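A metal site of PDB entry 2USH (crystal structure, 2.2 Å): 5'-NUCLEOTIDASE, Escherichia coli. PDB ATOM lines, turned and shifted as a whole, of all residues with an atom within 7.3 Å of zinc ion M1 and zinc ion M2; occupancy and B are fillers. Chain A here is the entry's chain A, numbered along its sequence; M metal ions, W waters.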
ATOM      1  N   ASN A  40      -6.276  12.623   8.552  1.00  0.00           N
ATOM      2  CA  ASN A  40      -6.890  11.655   7.645  1.00  0.00           C
ATOM      3  C   ASN A  40      -6.160  11.616   6.324  1.00  0.00           C
ATOM      4  O   ASN A  40      -5.424  12.534   6.002  1.00  0.00           O
ATOM      5  CB  ASN A  40      -8.353  12.020   7.360  1.00  0.00           C
ATOM      6  CG  ASN A  40      -8.490  13.424   6.852  1.00  0.00           C
ATOM      7  OD1 ASN A  40      -8.412  14.394   7.630  1.00  0.00           O
ATOM      8  ND2 ASN A  40      -8.672  13.559   5.542  1.00  0.00           N
ATOM      9  N   ASP A  41      -6.359  10.538   5.574  1.00  0.00           N
ATOM     10  CA  ASP A  41      -5.769  10.409   4.247  1.00  0.00           C
ATOM     11  C   ASP A  41      -4.285  10.729   4.176  1.00  0.00           C
ATOM     12  O   ASP A  41      -3.833  11.531   3.352  1.00  0.00           O
ATOM     13  CB  ASP A  41      -6.578  11.289   3.328  1.00  0.00           C
ATOM     14  CG  ASP A  41      -8.024  10.875   3.334  1.00  0.00           C
ATOM     15  OD1 ASP A  41      -8.809  11.357   4.186  1.00  0.00           O
ATOM     16  OD2 ASP A  41      -8.343  10.006   2.504  1.00  0.00           O
ATOM     17  N   HIS A  42      -3.569  10.064   5.076  1.00  0.00           N
ATOM     18  CA  HIS A  42      -2.128  10.110   5.253  1.00  0.00           C
ATOM     19  C   HIS A  42      -1.441   9.681   3.958  1.00  0.00           C
ATOM     20  O   HIS A  42      -0.470  10.291   3.528  1.00  0.00           O
ATOM     21  CB  HIS A  42      -1.743   9.171   6.408  1.00  0.00           C
ATOM     22  CG  HIS A  42      -0.264   9.080   6.633  1.00  0.00           C
ATOM     23  ND1 HIS A  42       0.473  10.146   7.081  1.00  0.00           N
ATOM     24  CD2 HIS A  42       0.605   8.075   6.385  1.00  0.00           C
ATOM     25  CE1 HIS A  42       1.754   9.809   7.096  1.00  0.00           C
ATOM     26  NE2 HIS A  42       1.861   8.560   6.671  1.00  0.00           N
ATOM     27  N   HIS A  43      -1.958   8.613   3.357  1.00  0.00           N
ATOM     28  CA  HIS A  43      -1.442   8.108   2.096  1.00  0.00           C
ATOM     29  C   HIS A  43       0.070   7.953   1.834  1.00  0.00           C
ATOM     30  O   HIS A  43       0.568   8.403   0.820  1.00  0.00           O
ATOM     31  CB  HIS A  43      -2.087   8.887   0.928  1.00  0.00           C
ATOM     32  CG  HIS A  43      -3.548   8.586   0.736  1.00  0.00           C
ATOM     33  ND1 HIS A  43      -4.024   7.303   0.580  1.00  0.00           N
ATOM     34  CD2 HIS A  43      -4.623   9.396   0.628  1.00  0.00           C
ATOM     35  CE1 HIS A  43      -5.322   7.331   0.381  1.00  0.00           C
ATOM     36  NE2 HIS A  43      -5.721   8.592   0.415  1.00  0.00           N
ATOM     37  N   GLY A  82      -8.902   9.527  10.319  1.00  0.00           N
ATOM     38  CA  GLY A  82     -10.017   9.235   9.429  1.00  0.00           C
ATOM     39  C   GLY A  82      -9.696   8.182   8.358  1.00  0.00           C
ATOM     40  O   GLY A  82     -10.467   8.030   7.396  1.00  0.00           O
ATOM     41  N   GLY A  83      -8.569   7.472   8.472  1.00  0.00           N
ATOM     42  CA  GLY A  83      -8.269   6.436   7.495  1.00  0.00           C
ATOM     43  C   GLY A  83      -7.440   6.798   6.270  1.00  0.00           C
ATOM     44  O   GLY A  83      -7.059   7.956   6.099  1.00  0.00           O
ATOM     45  N   ASP A  84      -7.258   5.827   5.372  1.00  0.00           N
ATOM     46  CA  ASP A  84      -6.396   5.964   4.180  1.00  0.00           C
ATOM     47  C   ASP A  84      -4.934   6.272   4.519  1.00  0.00           C
ATOM     48  O   ASP A  84      -4.403   7.329   4.204  1.00  0.00           O
ATOM     49  CB  ASP A  84      -6.934   6.967   3.162  1.00  0.00           C
ATOM     50  CG  ASP A  84      -7.985   6.365   2.255  1.00  0.00           C
ATOM     51  OD1 ASP A  84      -8.254   5.160   2.383  1.00  0.00           O
ATOM     52  OD2 ASP A  84      -8.521   7.071   1.383  1.00  0.00           O
ATOM     53  N   ILE A  85      -4.301   5.312   5.182  1.00  0.00           N
ATOM     54  CA  ILE A  85      -2.917   5.410   5.578  1.00  0.00           C
ATOM     55  C   ILE A  85      -2.140   4.855   4.386  1.00  0.00           C
ATOM     56  O   ILE A  85      -1.046   5.316   4.066  1.00  0.00           O
ATOM     57  CB  ILE A  85      -2.654   4.510   6.826  1.00  0.00           C
ATOM     58  CG1 ILE A  85      -3.677   4.874   7.902  1.00  0.00           C
ATOM     59  CG2 ILE A  85      -1.211   4.644   7.305  1.00  0.00           C
ATOM     60  CD1 ILE A  85      -3.715   6.334   8.266  1.00  0.00           C
ATOM     61  N   ASN A  86      -2.731   3.850   3.738  1.00  0.00           N
ATOM     62  CA  ASN A  86      -2.189   3.172   2.563  1.00  0.00           C
ATOM     63  C   ASN A  86      -2.292   3.935   1.260  1.00  0.00           C
ATOM     64  O   ASN A  86      -3.228   4.706   1.043  1.00  0.00           O
ATOM     65  CB  ASN A  86      -2.891   1.809   2.316  1.00  0.00           C
ATOM     66  CG  ASN A  86      -2.483   0.716   3.307  1.00  0.00           C
ATOM     67  OD1 ASN A  86      -1.505   0.015   3.078  1.00  0.00           O
ATOM     68  ND2 ASN A  86      -3.244   0.528   4.378  1.00  0.00           N
ATOM     69  N   THR A  87      -1.316   3.672   0.391  1.00  0.00           N
ATOM     70  CA  THR A  87      -1.268   4.174  -0.990  1.00  0.00           C
ATOM     71  C   THR A  87      -1.006   5.643  -1.222  1.00  0.00           C
ATOM     72  O   THR A  87      -1.794   6.473  -0.835  1.00  0.00           O
ATOM     73  CB  THR A  87      -2.569   3.821  -1.687  1.00  0.00           C
ATOM     74  OG1 THR A  87      -2.795   2.400  -1.552  1.00  0.00           O
ATOM     75  CG2 THR A  87      -2.518   4.193  -3.167  1.00  0.00           C
ATOM     76  N   GLY A 115     -10.155   3.122   5.890  1.00  0.00           N
ATOM     77  CA  GLY A 115     -10.469   3.801   4.642  1.00  0.00           C
ATOM     78  C   GLY A 115     -10.597   2.885   3.433  1.00  0.00           C
ATOM     79  O   GLY A 115     -10.302   1.696   3.494  1.00  0.00           O
ATOM     80  N   ASN A 116     -11.049   3.427   2.308  1.00  0.00           N
ATOM     81  CA  ASN A 116     -11.193   2.601   1.139  1.00  0.00           C
ATOM     82  C   ASN A 116      -9.835   2.083   0.644  1.00  0.00           C
ATOM     83  O   ASN A 116      -9.748   0.979   0.126  1.00  0.00           O
ATOM     84  CB  ASN A 116     -11.966   3.363   0.042  1.00  0.00           C
ATOM     85  CG  ASN A 116     -11.263   4.632  -0.396  1.00  0.00           C
ATOM     86  OD1 ASN A 116     -10.911   5.476   0.414  1.00  0.00           O
ATOM     87  ND2 ASN A 116     -11.075   4.782  -1.706  1.00  0.00           N
ATOM     88  N   HIS A 117      -8.772   2.859   0.818  1.00  0.00           N
ATOM     89  CA  HIS A 117      -7.452   2.393   0.374  1.00  0.00           C
ATOM     90  C   HIS A 117      -6.730   1.378   1.276  1.00  0.00           C
ATOM     91  O   HIS A 117      -5.579   1.013   0.992  1.00  0.00           O
ATOM     92  CB  HIS A 117      -6.499   3.564   0.041  1.00  0.00           C
ATOM     93  CG  HIS A 117      -6.867   4.287  -1.221  1.00  0.00           C
ATOM     94  ND1 HIS A 117      -6.514   3.817  -2.470  1.00  0.00           N
ATOM     95  CD2 HIS A 117      -7.632   5.388  -1.441  1.00  0.00           C
ATOM     96  CE1 HIS A 117      -7.062   4.572  -3.402  1.00  0.00           C
ATOM     97  NE2 HIS A 117      -7.736   5.531  -2.805  1.00  0.00           N
ATOM     98  N   THR A 172     -16.744   4.132   3.837  1.00  0.00           N
ATOM     99  CA  THR A 172     -17.550   4.355   2.630  1.00  0.00           C
ATOM    100  C   THR A 172     -17.860   3.048   1.917  1.00  0.00           C
ATOM    101  O   THR A 172     -16.998   2.185   1.723  1.00  0.00           O
ATOM    102  CB  THR A 172     -16.855   5.322   1.607  1.00  0.00           C
ATOM    103  OG1 THR A 172     -17.722   5.489   0.477  1.00  0.00           O
ATOM    104  CG2 THR A 172     -15.518   4.776   1.142  1.00  0.00           C
ATOM    105  N   THR A 175     -16.151   1.705  -1.497  1.00  0.00           N
ATOM    106  CA  THR A 175     -14.905   0.976  -1.526  1.00  0.00           C
ATOM    107  C   THR A 175     -14.918  -0.127  -2.546  1.00  0.00           C
ATOM    108  O   THR A 175     -13.911  -0.356  -3.168  1.00  0.00           O
ATOM    109  CB  THR A 175     -14.570   0.437  -0.134  1.00  0.00           C
ATOM    110  OG1 THR A 175     -14.361   1.563   0.732  1.00  0.00           O
ATOM    111  CG2 THR A 175     -13.302  -0.457  -0.171  1.00  0.00           C
ATOM    112  N   HIS A 217     -14.774   7.347   7.171  1.00  0.00           N
ATOM    113  CA  HIS A 217     -14.045   7.578   5.934  1.00  0.00           C
ATOM    114  C   HIS A 217     -15.112   7.597   4.826  1.00  0.00           C
ATOM    115  O   HIS A 217     -15.232   6.668   4.031  1.00  0.00           O
ATOM    116  CB  HIS A 217     -13.029   6.485   5.722  1.00  0.00           C
ATOM    117  CG  HIS A 217     -12.082   6.815   4.637  1.00  0.00           C
ATOM    118  ND1 HIS A 217     -10.957   7.573   4.877  1.00  0.00           N
ATOM    119  CD2 HIS A 217     -12.151   6.631   3.303  1.00  0.00           C
ATOM    120  CE1 HIS A 217     -10.380   7.853   3.725  1.00  0.00           C
ATOM    121  NE2 HIS A 217     -11.092   7.305   2.755  1.00  0.00           N
ATOM    122  N   MET A 218     -15.881   8.695   4.795  1.00  0.00           N
ATOM    123  CA  MET A 218     -17.021   8.822   3.878  1.00  0.00           C
ATOM    124  C   MET A 218     -17.029  10.069   2.985  1.00  0.00           C
ATOM    125  O   MET A 218     -17.598  10.036   1.904  1.00  0.00           O
ATOM    126  CB  MET A 218     -18.308   8.722   4.724  1.00  0.00           C
ATOM    127  CG  MET A 218     -18.416   7.373   5.505  1.00  0.00           C
ATOM    128  SD  MET A 218     -19.715   7.313   6.775  1.00  0.00           S
ATOM    129  CE  MET A 218     -21.065   8.220   6.010  1.00  0.00           C
ATOM    130  N   GLY A 251     -12.910  12.011   6.525  1.00  0.00           N
ATOM    131  CA  GLY A 251     -11.843  11.841   5.548  1.00  0.00           C
ATOM    132  C   GLY A 251     -12.392  11.467   4.182  1.00  0.00           C
ATOM    133  O   GLY A 251     -13.573  11.703   3.886  1.00  0.00           O
ATOM    134  N   HIS A 252     -11.528  10.925   3.341  1.00  0.00           N
ATOM    135  CA  HIS A 252     -11.888  10.432   2.026  1.00  0.00           C
ATOM    136  C   HIS A 252     -12.021  11.482   0.944  1.00  0.00           C
ATOM    137  O   HIS A 252     -11.398  11.366  -0.110  1.00  0.00           O
ATOM    138  CB  HIS A 252     -13.182   9.603   2.094  1.00  0.00           C
ATOM    139  CG  HIS A 252     -13.519   8.915   0.801  1.00  0.00           C
ATOM    140  ND1 HIS A 252     -12.631   8.089   0.158  1.00  0.00           N
ATOM    141  CD2 HIS A 252     -14.639   8.930   0.045  1.00  0.00           C
ATOM    142  CE1 HIS A 252     -13.186   7.625  -0.944  1.00  0.00           C
ATOM    143  NE2 HIS A 252     -14.395   8.117  -1.038  1.00  0.00           N
ATOM    144  N   SER A 253     -12.869  12.474   1.172  1.00  0.00           N
ATOM    145  CA  SER A 253     -13.012  13.552   0.208  1.00  0.00           C
ATOM    146  C   SER A 253     -11.714  14.381   0.206  1.00  0.00           C
ATOM    147  O   SER A 253     -11.407  15.018  -0.772  1.00  0.00           O
ATOM    148  CB  SER A 253     -14.235  14.438   0.523  1.00  0.00           C
ATOM    149  OG  SER A 253     -14.206  15.035   1.815  1.00  0.00           O
ATOM    150  N   GLN A 254     -10.966  14.364   1.316  1.00  0.00           N
ATOM    151  CA  GLN A 254      -9.706  15.079   1.459  1.00  0.00           C
ATOM    152  C   GLN A 254      -9.741  16.584   1.321  1.00  0.00           C
ATOM    153  O   GLN A 254      -8.976  17.171   0.564  1.00  0.00           O
ATOM    154  CB  GLN A 254      -8.659  14.486   0.513  1.00  0.00           C
ATOM    155  CG  GLN A 254      -8.412  13.019   0.835  1.00  0.00           C
ATOM    156  CD  GLN A 254      -7.418  12.359  -0.099  1.00  0.00           C
ATOM    157  OE1 GLN A 254      -7.511  11.162  -0.378  1.00  0.00           O
ATOM    158  NE2 GLN A 254      -6.446  13.137  -0.575  1.00  0.00           N
ATOM    159  N   HIS A 289      -7.994  17.622   5.539  1.00  0.00           N
ATOM    160  CA  HIS A 289      -7.404  17.616   4.230  1.00  0.00           C
ATOM    161  C   HIS A 289      -6.674  16.310   3.873  1.00  0.00           C
ATOM    162  O   HIS A 289      -7.327  15.301   3.597  1.00  0.00           O
ATOM    163  CB  HIS A 289      -6.465  18.817   4.150  1.00  0.00           C
ATOM    164  CG  HIS A 289      -5.927  19.073   2.790  1.00  0.00           C
ATOM    165  ND1 HIS A 289      -6.638  18.786   1.647  1.00  0.00           N
ATOM    166  CD2 HIS A 289      -4.763  19.638   2.382  1.00  0.00           C
ATOM    167  CE1 HIS A 289      -5.936  19.167   0.586  1.00  0.00           C
ATOM    168  NE2 HIS A 289      -4.801  19.693   1.014  1.00  0.00           N
ATOM    169  N   GLU A 290      -5.345  16.278   3.875  1.00  0.00           N
ATOM    170  CA  GLU A 290      -4.696  15.044   3.486  1.00  0.00           C
ATOM    171  C   GLU A 290      -3.201  15.131   3.755  1.00  0.00           C
ATOM    172  O   GLU A 290      -2.680  16.204   4.016  1.00  0.00           O
ATOM    173  CB  GLU A 290      -4.858  14.841   1.965  1.00  0.00           C
ATOM    174  CG  GLU A 290      -4.022  15.903   1.222  1.00  0.00           C
ATOM    175  CD  GLU A 290      -4.321  16.037  -0.246  1.00  0.00           C
ATOM    176  OE1 GLU A 290      -5.307  15.445  -0.725  1.00  0.00           O
ATOM    177  OE2 GLU A 290      -3.567  16.763  -0.913  1.00  0.00           O
ATOM    178  N   TRP A 291      -2.545  13.958   3.661  1.00  0.00           N
ATOM    179  CA  TRP A 291      -1.091  13.795   3.763  1.00  0.00           C
ATOM    180  C   TRP A 291      -0.305  14.281   4.981  1.00  0.00           C
ATOM    181  O   TRP A 291       0.910  14.481   4.882  1.00  0.00           O
ATOM    182  CB  TRP A 291      -0.430  14.428   2.525  1.00  0.00           C
ATOM    183  CG  TRP A 291      -0.934  13.898   1.197  1.00  0.00           C
ATOM    184  CD1 TRP A 291      -1.822  12.880   0.985  1.00  0.00           C
ATOM    185  CD2 TRP A 291      -0.591  14.418  -0.110  1.00  0.00           C
ATOM    186  NE1 TRP A 291      -2.054  12.729  -0.362  1.00  0.00           N
ATOM    187  CE2 TRP A 291      -1.313  13.660  -1.052  1.00  0.00           C
ATOM    188  CE3 TRP A 291       0.256  15.447  -0.565  1.00  0.00           C
ATOM    189  CZ2 TRP A 291      -1.218  13.900  -2.448  1.00  0.00           C
ATOM    190  CZ3 TRP A 291       0.355  15.684  -1.944  1.00  0.00           C
ATOM    191  CH2 TRP A 291      -0.383  14.903  -2.869  1.00  0.00           C
ATOM    192  N   THR A 518      -9.610   8.553  -8.102  1.00  0.00           N
ATOM    193  CA  THR A 518      -9.322   7.209  -7.555  1.00  0.00           C
ATOM    194  C   THR A 518      -8.317   7.194  -6.430  1.00  0.00           C
ATOM    195  O   THR A 518      -8.246   6.237  -5.684  1.00  0.00           O
ATOM    196  CB  THR A 518      -8.769   6.255  -8.604  1.00  0.00           C
ATOM    197  OG1 THR A 518      -7.491   6.753  -9.055  1.00  0.00           O
ATOM    198  CG2 THR A 518      -9.724   6.155  -9.788  1.00  0.00           C
ATOM    199  N   GLY A 519      -7.524   8.244  -6.309  1.00  0.00           N
ATOM    200  CA  GLY A 519      -6.522   8.205  -5.273  1.00  0.00           C
ATOM    201  C   GLY A 519      -5.316   7.370  -5.713  1.00  0.00           C
ATOM    202  O   GLY A 519      -4.401   7.202  -4.923  1.00  0.00           O
HETATM  203 ZN    ZN M   1      -7.813   9.156   0.644  1.00  0.00          ZN
HETATM  204 ZN    ZN M   2     -10.653   7.419   0.749  1.00  0.00          ZN
HETATM  205  O   HOH W   1      -9.529   8.809  -0.414  1.00  0.00           O
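Zinc ion M1 is bound by water W1 (2.0 Å), the side-chain carboxylate (OD2) of Asp 41 (2.1 Å), a ring nitrogen (NE2) of His 43 (2.2 Å), the side-chain amide oxygen (OE1) of Gln 254 (2.3 Å) and the side-chain carboxylate (OD2) of Asp 84 (2.3 Å).
A ring nitrogen (ND1) of His 217 lies within hydrogen-bond range of the backbone carbonyl oxygen (O) of Gly 82 (2.6 Å). A ring nitrogen (ND1) of His 43 is in hydrogen-bond range of the backbone carbonyl oxygen (O) of Asn 86, at 2.8 Å. The side-chain carboxylate of Asp 84 sits at hydrogen-bond distance from the backbone NH of His 117, 2.8 Å away. The backbone carbonyl oxygen (O) of Gln 254 lies within hydrogen-bond range of a ring nitrogen (ND1) of His 289 (3.0 Å). The backbone NH (N) of His 43 sits close to the backbone carbonyl oxygen (O) of Ile 85 (3.5 Å). ND1 of His 43 is in hydrogen-bond range of O of Thr 87 (2.8 Å). The side-chain amide nitrogen of Gln 254 sits at hydrogen-bond distance from the side-chain carboxylate of Glu 290 (2.6 Å). The backbone carbonyl oxygen of Gly 83 sits at hydrogen-bond distance from the backbone NH of Asp 41, 2.7 Å away.
OD1 of Asn 116 is bound to zinc ion M2, 2.0 Å away. NE2 of His 217 is bound to zinc ion M2. Water W1 is bound to zinc ion M2 (2.1 Å). ND1 of His 252 binds zinc ion M2, 2.2 Å away. OD2 of Asp 84 binds zinc ion M2, 2.3 Å away.
Of the 26 residues printed, 4 come within 4 Å of zinc ion M1. The nearest printed residue that does not touch zinc ion M1 is His 217 (4.2 Å).
Of the 26 residues printed, 5 come within 4 Å of zinc ion M2.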
